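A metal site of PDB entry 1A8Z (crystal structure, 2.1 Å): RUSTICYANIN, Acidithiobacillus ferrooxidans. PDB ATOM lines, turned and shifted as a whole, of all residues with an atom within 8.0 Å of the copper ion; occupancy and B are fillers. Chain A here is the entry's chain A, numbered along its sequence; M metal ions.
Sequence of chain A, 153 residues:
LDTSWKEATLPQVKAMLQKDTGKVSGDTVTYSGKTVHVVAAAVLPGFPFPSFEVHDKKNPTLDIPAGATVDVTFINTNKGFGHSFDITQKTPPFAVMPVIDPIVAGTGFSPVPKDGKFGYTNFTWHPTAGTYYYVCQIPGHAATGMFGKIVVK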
ATOM      1  N   ALA A  42       2.674 -20.158  23.601  1.00  0.00           N
ATOM      2  CA  ALA A  42       3.929 -20.793  23.197  1.00  0.00           C
ATOM      3  C   ALA A  42       4.509 -20.031  22.013  1.00  0.00           C
ATOM      4  O   ALA A  42       3.892 -19.998  20.956  1.00  0.00           O
ATOM      5  CB  ALA A  42       3.653 -22.223  22.789  1.00  0.00           C
ATOM      6  N   VAL A  43       5.670 -19.419  22.224  1.00  0.00           N
ATOM      7  CA  VAL A  43       6.425 -18.667  21.196  1.00  0.00           C
ATOM      8  C   VAL A  43       5.593 -17.693  20.356  1.00  0.00           C
ATOM      9  O   VAL A  43       5.124 -18.030  19.266  1.00  0.00           O
ATOM     10  CB  VAL A  43       7.215 -19.610  20.231  1.00  0.00           C
ATOM     11  CG1 VAL A  43       8.387 -18.862  19.649  1.00  0.00           C
ATOM     12  CG2 VAL A  43       7.725 -20.856  20.977  1.00  0.00           C
ATOM     13  N   PHE A  49      12.708 -18.882  20.294  1.00  0.00           N
ATOM     14  CA  PHE A  49      12.268 -20.275  20.267  1.00  0.00           C
ATOM     15  C   PHE A  49      13.290 -21.108  21.077  1.00  0.00           C
ATOM     16  O   PHE A  49      14.512 -20.858  20.989  1.00  0.00           O
ATOM     17  CB  PHE A  49      12.210 -20.805  18.831  1.00  0.00           C
ATOM     18  CG  PHE A  49      11.830 -22.270  18.725  1.00  0.00           C
ATOM     19  CD1 PHE A  49      12.798 -23.269  18.853  1.00  0.00           C
ATOM     20  CD2 PHE A  49      10.500 -22.642  18.555  1.00  0.00           C
ATOM     21  CE1 PHE A  49      12.440 -24.605  18.814  1.00  0.00           C
ATOM     22  CE2 PHE A  49      10.139 -23.987  18.506  1.00  0.00           C
ATOM     23  CZ  PHE A  49      11.111 -24.964  18.640  1.00  0.00           C
ATOM     24  N   PRO A  50      12.811 -21.982  22.011  1.00  0.00           N
ATOM     25  CA  PRO A  50      11.400 -22.210  22.346  1.00  0.00           C
ATOM     26  C   PRO A  50      11.155 -21.480  23.664  1.00  0.00           C
ATOM     27  O   PRO A  50      12.047 -21.437  24.522  1.00  0.00           O
ATOM     28  CB  PRO A  50      11.346 -23.727  22.511  1.00  0.00           C
ATOM     29  CG  PRO A  50      12.646 -24.038  23.154  1.00  0.00           C
ATOM     30  CD  PRO A  50      13.654 -23.083  22.508  1.00  0.00           C
ATOM     31  N   SER A  51       9.977 -20.910  23.849  1.00  0.00           N
ATOM     32  CA  SER A  51       9.727 -20.191  25.083  1.00  0.00           C
ATOM     33  C   SER A  51       8.236 -19.970  25.315  1.00  0.00           C
ATOM     34  O   SER A  51       7.418 -20.191  24.401  1.00  0.00           O
ATOM     35  CB  SER A  51      10.439 -18.821  25.028  1.00  0.00           C
ATOM     36  OG  SER A  51       9.845 -17.978  24.031  1.00  0.00           O
ATOM     37  N   PHE A  52       7.884 -19.593  26.545  1.00  0.00           N
ATOM     38  CA  PHE A  52       6.505 -19.294  26.890  1.00  0.00           C
ATOM     39  C   PHE A  52       6.462 -17.774  27.102  1.00  0.00           C
ATOM     40  O   PHE A  52       7.430 -17.165  27.524  1.00  0.00           O
ATOM     41  CB  PHE A  52       6.092 -19.958  28.213  1.00  0.00           C
ATOM     42  CG  PHE A  52       5.874 -21.428  28.126  1.00  0.00           C
ATOM     43  CD1 PHE A  52       4.793 -21.948  27.433  1.00  0.00           C
ATOM     44  CD2 PHE A  52       6.713 -22.311  28.804  1.00  0.00           C
ATOM     45  CE1 PHE A  52       4.537 -23.311  27.423  1.00  0.00           C
ATOM     46  CE2 PHE A  52       6.470 -23.668  28.793  1.00  0.00           C
ATOM     47  CZ  PHE A  52       5.379 -24.170  28.106  1.00  0.00           C
ATOM     48  N   PHE A  74      -4.068 -21.545  27.770  1.00  0.00           N
ATOM     49  CA  PHE A  74      -2.820 -21.758  27.068  1.00  0.00           C
ATOM     50  C   PHE A  74      -3.152 -21.772  25.559  1.00  0.00           C
ATOM     51  O   PHE A  74      -4.115 -22.422  25.126  1.00  0.00           O
ATOM     52  CB  PHE A  74      -2.170 -23.073  27.525  1.00  0.00           C
ATOM     53  CG  PHE A  74      -0.970 -23.478  26.693  1.00  0.00           C
ATOM     54  CD1 PHE A  74       0.177 -22.692  26.670  1.00  0.00           C
ATOM     55  CD2 PHE A  74      -0.999 -24.643  25.926  1.00  0.00           C
ATOM     56  CE1 PHE A  74       1.280 -23.059  25.891  1.00  0.00           C
ATOM     57  CE2 PHE A  74       0.091 -25.017  25.148  1.00  0.00           C
ATOM     58  CZ  PHE A  74       1.240 -24.220  25.134  1.00  0.00           C
ATOM     59  N   ASN A  76      -1.297 -22.112  21.642  1.00  0.00           N
ATOM     60  CA  ASN A  76      -0.080 -22.468  20.901  1.00  0.00           C
ATOM     61  C   ASN A  76      -0.069 -21.638  19.590  1.00  0.00           C
ATOM     62  O   ASN A  76      -0.848 -21.921  18.677  1.00  0.00           O
ATOM     63  CB  ASN A  76      -0.084 -23.962  20.570  1.00  0.00           C
ATOM     64  CG  ASN A  76       1.081 -24.361  19.701  1.00  0.00           C
ATOM     65  OD1 ASN A  76       0.988 -25.279  18.901  1.00  0.00           O
ATOM     66  ND2 ASN A  76       2.180 -23.663  19.839  1.00  0.00           N
ATOM     67  N   ASN A  78       2.833 -21.151  17.803  1.00  0.00           N
ATOM     68  CA  ASN A  78       4.049 -21.519  17.096  1.00  0.00           C
ATOM     69  C   ASN A  78       3.790 -22.544  16.008  1.00  0.00           C
ATOM     70  O   ASN A  78       3.497 -23.715  16.279  1.00  0.00           O
ATOM     71  CB  ASN A  78       5.080 -22.068  18.087  1.00  0.00           C
ATOM     72  CG  ASN A  78       6.465 -22.139  17.518  1.00  0.00           C
ATOM     73  OD1 ASN A  78       6.922 -21.227  16.826  1.00  0.00           O
ATOM     74  ND2 ASN A  78       7.161 -23.225  17.813  1.00  0.00           N
ATOM     75  N   PHE A  81       4.847 -26.823  15.630  1.00  0.00           N
ATOM     76  CA  PHE A  81       5.047 -27.556  16.896  1.00  0.00           C
ATOM     77  C   PHE A  81       3.801 -27.570  17.799  1.00  0.00           C
ATOM     78  O   PHE A  81       3.086 -26.560  17.886  1.00  0.00           O
ATOM     79  CB  PHE A  81       6.228 -26.947  17.685  1.00  0.00           C
ATOM     80  CG  PHE A  81       7.489 -26.846  16.898  1.00  0.00           C
ATOM     81  CD1 PHE A  81       7.699 -25.769  16.033  1.00  0.00           C
ATOM     82  CD2 PHE A  81       8.449 -27.851  16.960  1.00  0.00           C
ATOM     83  CE1 PHE A  81       8.845 -25.707  15.260  1.00  0.00           C
ATOM     84  CE2 PHE A  81       9.590 -27.795  16.194  1.00  0.00           C
ATOM     85  CZ  PHE A  81       9.790 -26.714  15.338  1.00  0.00           C
ATOM     86  N   GLY A  82       3.570 -28.708  18.460  1.00  0.00           N
ATOM     87  CA  GLY A  82       2.431 -28.856  19.365  1.00  0.00           C
ATOM     88  C   GLY A  82       2.928 -28.888  20.808  1.00  0.00           C
ATOM     89  O   GLY A  82       2.910 -29.930  21.469  1.00  0.00           O
ATOM     90  N   HIS A  83       3.381 -27.753  21.284  1.00  0.00           N
ATOM     91  CA  HIS A  83       3.890 -27.625  22.648  1.00  0.00           C
ATOM     92  C   HIS A  83       2.809 -27.973  23.685  1.00  0.00           C
ATOM     93  O   HIS A  83       1.630 -28.010  23.364  1.00  0.00           O
ATOM     94  CB  HIS A  83       4.322 -26.180  22.896  1.00  0.00           C
ATOM     95  CG  HIS A  83       5.251 -25.628  21.859  1.00  0.00           C
ATOM     96  ND1 HIS A  83       6.609 -25.858  21.880  1.00  0.00           N
ATOM     97  CD2 HIS A  83       5.029 -24.782  20.815  1.00  0.00           C
ATOM     98  CE1 HIS A  83       7.182 -25.167  20.901  1.00  0.00           C
ATOM     99  NE2 HIS A  83       6.244 -24.507  20.248  1.00  0.00           N
ATOM    100  N   SER A  84       3.253 -28.189  24.928  1.00  0.00           N
ATOM    101  CA  SER A  84       2.367 -28.480  26.054  1.00  0.00           C
ATOM    102  C   SER A  84       2.690 -27.472  27.151  1.00  0.00           C
ATOM    103  O   SER A  84       3.728 -26.817  27.111  1.00  0.00           O
ATOM    104  CB  SER A  84       2.599 -29.907  26.604  1.00  0.00           C
ATOM    105  OG  SER A  84       3.885 -30.037  27.206  1.00  0.00           O
ATOM    106  N   PHE A  85       1.757 -27.292  28.086  1.00  0.00           N
ATOM    107  CA  PHE A  85       1.959 -26.386  29.234  1.00  0.00           C
ATOM    108  C   PHE A  85       1.664 -27.269  30.447  1.00  0.00           C
ATOM    109  O   PHE A  85       0.514 -27.622  30.676  1.00  0.00           O
ATOM    110  CB  PHE A  85       0.949 -25.237  29.193  1.00  0.00           C
ATOM    111  CG  PHE A  85       1.198 -24.180  30.240  1.00  0.00           C
ATOM    112  CD1 PHE A  85       2.087 -23.148  29.992  1.00  0.00           C
ATOM    113  CD2 PHE A  85       0.521 -24.224  31.471  1.00  0.00           C
ATOM    114  CE1 PHE A  85       2.303 -22.170  30.943  1.00  0.00           C
ATOM    115  CE2 PHE A  85       0.748 -23.234  32.437  1.00  0.00           C
ATOM    116  CZ  PHE A  85       1.635 -22.199  32.176  1.00  0.00           C
ATOM    117  N   PHE A 109      -0.348 -32.499  24.539  1.00  0.00           N
ATOM    118  CA  PHE A 109       0.324 -31.771  23.459  1.00  0.00           C
ATOM    119  C   PHE A 109      -0.754 -31.049  22.614  1.00  0.00           C
ATOM    120  O   PHE A 109      -1.790 -31.645  22.264  1.00  0.00           O
ATOM    121  CB  PHE A 109       1.140 -32.731  22.588  1.00  0.00           C
ATOM    122  CG  PHE A 109       2.337 -33.305  23.269  1.00  0.00           C
ATOM    123  CD1 PHE A 109       3.386 -32.499  23.677  1.00  0.00           C
ATOM    124  CD2 PHE A 109       2.422 -34.687  23.520  1.00  0.00           C
ATOM    125  CE1 PHE A 109       4.507 -33.051  24.315  1.00  0.00           C
ATOM    126  CE2 PHE A 109       3.524 -35.233  24.148  1.00  0.00           C
ATOM    127  CZ  PHE A 109       4.571 -34.423  24.543  1.00  0.00           C
ATOM    128  N   SER A 110      -0.560 -29.762  22.334  1.00  0.00           N
ATOM    129  CA  SER A 110      -1.528 -28.986  21.568  1.00  0.00           C
ATOM    130  C   SER A 110      -1.522 -29.225  20.056  1.00  0.00           C
ATOM    131  O   SER A 110      -0.565 -29.764  19.506  1.00  0.00           O
ATOM    132  CB  SER A 110      -1.272 -27.508  21.762  1.00  0.00           C
ATOM    133  OG  SER A 110       0.026 -27.174  21.285  1.00  0.00           O
ATOM    134  N   VAL A 135       6.310 -26.219  32.322  1.00  0.00           N
ATOM    135  CA  VAL A 135       7.250 -26.711  31.316  1.00  0.00           C
ATOM    136  C   VAL A 135       6.554 -27.244  30.084  1.00  0.00           C
ATOM    137  O   VAL A 135       5.355 -27.508  30.106  1.00  0.00           O
ATOM    138  CB  VAL A 135       8.119 -27.905  31.852  1.00  0.00           C
ATOM    139  CG1 VAL A 135       8.880 -27.546  33.111  1.00  0.00           C
ATOM    140  CG2 VAL A 135       7.223 -29.110  32.116  1.00  0.00           C
ATOM    141  N   CYS A 136       7.325 -27.407  29.023  1.00  0.00           N
ATOM    142  CA  CYS A 136       6.801 -28.013  27.814  1.00  0.00           C
ATOM    143  C   CYS A 136       7.386 -29.419  27.808  1.00  0.00           C
ATOM    144  O   CYS A 136       8.573 -29.601  28.095  1.00  0.00           O
ATOM    145  CB  CYS A 136       7.292 -27.296  26.559  1.00  0.00           C
ATOM    146  SG  CYS A 136       6.706 -28.116  25.047  1.00  0.00           S
ATOM    147  N   GLN A 137       6.578 -30.399  27.446  1.00  0.00           N
ATOM    148  CA  GLN A 137       7.019 -31.788  27.414  1.00  0.00           C
ATOM    149  C   GLN A 137       7.650 -32.264  26.096  1.00  0.00           C
ATOM    150  O   GLN A 137       8.068 -33.424  26.008  1.00  0.00           O
ATOM    151  CB  GLN A 137       5.869 -32.725  27.790  1.00  0.00           C
ATOM    152  CG  GLN A 137       5.624 -32.873  29.292  1.00  0.00           C
ATOM    153  CD  GLN A 137       4.837 -34.148  29.618  1.00  0.00           C
ATOM    154  OE1 GLN A 137       3.599 -34.169  29.553  1.00  0.00           O
ATOM    155  NE2 GLN A 137       5.549 -35.217  29.922  1.00  0.00           N
ATOM    156  N   ILE A 138       7.682 -31.419  25.059  1.00  0.00           N
ATOM    157  CA  ILE A 138       8.289 -31.858  23.805  1.00  0.00           C
ATOM    158  C   ILE A 138       9.760 -32.085  24.061  1.00  0.00           C
ATOM    159  O   ILE A 138      10.462 -31.187  24.544  1.00  0.00           O
ATOM    160  CB  ILE A 138       8.118 -30.838  22.666  1.00  0.00           C
ATOM    161  CG1 ILE A 138       6.655 -30.774  22.243  1.00  0.00           C
ATOM    162  CG2 ILE A 138       8.961 -31.256  21.464  1.00  0.00           C
ATOM    163  CD1 ILE A 138       6.400 -29.760  21.136  1.00  0.00           C
ATOM    164  N   PRO A 139      10.272 -33.282  23.729  1.00  0.00           N
ATOM    165  CA  PRO A 139      11.686 -33.615  23.937  1.00  0.00           C
ATOM    166  C   PRO A 139      12.667 -32.504  23.556  1.00  0.00           C
ATOM    167  O   PRO A 139      12.658 -32.001  22.431  1.00  0.00           O
ATOM    168  CB  PRO A 139      11.865 -34.866  23.080  1.00  0.00           C
ATOM    169  CG  PRO A 139      10.531 -35.531  23.191  1.00  0.00           C
ATOM    170  CD  PRO A 139       9.549 -34.392  23.078  1.00  0.00           C
ATOM    171  N   GLY A 140      13.508 -32.109  24.510  1.00  0.00           N
ATOM    172  CA  GLY A 140      14.489 -31.071  24.280  1.00  0.00           C
ATOM    173  C   GLY A 140      14.064 -29.626  24.522  1.00  0.00           C
ATOM    174  O   GLY A 140      14.941 -28.757  24.684  1.00  0.00           O
ATOM    175  N   HIS A 141      12.766 -29.324  24.554  1.00  0.00           N
ATOM    176  CA  HIS A 141      12.337 -27.935  24.783  1.00  0.00           C
ATOM    177  C   HIS A 141      12.608 -27.389  26.176  1.00  0.00           C
ATOM    178  O   HIS A 141      13.096 -26.273  26.304  1.00  0.00           O
ATOM    179  CB  HIS A 141      10.878 -27.753  24.433  1.00  0.00           C
ATOM    180  CG  HIS A 141      10.624 -27.762  22.958  1.00  0.00           C
ATOM    181  ND1 HIS A 141       9.373 -27.542  22.418  1.00  0.00           N
ATOM    182  CD2 HIS A 141      11.415 -28.120  21.919  1.00  0.00           C
ATOM    183  CE1 HIS A 141       9.400 -27.783  21.123  1.00  0.00           C
ATOM    184  NE2 HIS A 141      10.621 -28.132  20.796  1.00  0.00           N
ATOM    185  N   ALA A 142      12.281 -28.138  27.215  1.00  0.00           N
ATOM    186  CA  ALA A 142      12.549 -27.680  28.587  1.00  0.00           C
ATOM    187  C   ALA A 142      14.056 -27.603  28.825  1.00  0.00           C
ATOM    188  O   ALA A 142      14.554 -26.661  29.430  1.00  0.00           O
ATOM    189  CB  ALA A 142      11.885 -28.595  29.611  1.00  0.00           C
ATOM    190  N   THR A 144      16.231 -26.856  26.725  1.00  0.00           N
ATOM    191  CA  THR A 144      16.757 -25.657  26.086  1.00  0.00           C
ATOM    192  C   THR A 144      16.101 -24.374  26.572  1.00  0.00           C
ATOM    193  O   THR A 144      16.208 -23.349  25.923  1.00  0.00           O
ATOM    194  CB  THR A 144      16.699 -25.741  24.534  1.00  0.00           C
ATOM    195  OG1 THR A 144      15.353 -25.860  24.100  1.00  0.00           O
ATOM    196  CG2 THR A 144      17.473 -26.962  24.039  1.00  0.00           C
ATOM    197  N   MET A 146      12.517 -23.851  27.676  1.00  0.00           N
ATOM    198  CA  MET A 146      11.083 -23.595  27.673  1.00  0.00           C
ATOM    199  C   MET A 146      10.430 -23.977  29.014  1.00  0.00           C
ATOM    200  O   MET A 146       9.798 -25.019  29.118  1.00  0.00           O
ATOM    201  CB  MET A 146      10.418 -24.310  26.508  1.00  0.00           C
ATOM    202  CG  MET A 146       9.078 -23.739  26.150  1.00  0.00           C
ATOM    203  SD  MET A 146       8.394 -24.400  24.649  1.00  0.00           S
ATOM    204  CE  MET A 146       6.815 -23.689  24.671  1.00  0.00           C
HETATM  205 CU    CU M   1       7.672 -26.915  23.402  1.00  0.00          CU
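Ile 138 touches the copper ion (CD1 to CU, 3.9 Å).
Five residues have an atom within 4 Å of the copper ion: His 83, Cys 136, Ile 138, His 141 and Met 146.
The nearest printed residue that does not touch the copper ion is Ser 84 (4.8 Å).
The copper ion is bound by a ring nitrogen (ND1) of His 141, a ring nitrogen (ND1) of His 83 and the side-chain sulfur of Cys 136.
The copper ion has three donor atoms within binding distance.
Slightly farther from the copper ion lies the side-chain sulfur (SD) of Met 146 (2.9 Å).
N of Met 146 is in hydrogen-bond range of O of His 141, 2.8 Å away.
The backbone carbonyl oxygen (O) of His 141 sits at hydrogen-bond distance from the side-chain hydroxyl (OG1) of Thr 144, at 3.2 Å.
ND1 of His 83 sits close to SD of Met 146 (3.6 Å).
A ring nitrogen (NE2) of His 83 lies within hydrogen-bond range of the side-chain amide nitrogen of Asn 78, at 2.9 Å.
OG of Ser 110 lies within hydrogen-bond range of O of His 83, at 2.8 Å.
The backbone NH of Cys 136 is in hydrogen-bond range of the backbone carbonyl oxygen of Met 146 (3.4 Å).
The side-chain sulfur (SG) of Cys 136 lies close to the backbone NH (N) of Ile 138.
The side-chain sulfur (SG) of Cys 136 lies close to the backbone NH (N) of Ser 84 (3.5 Å).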
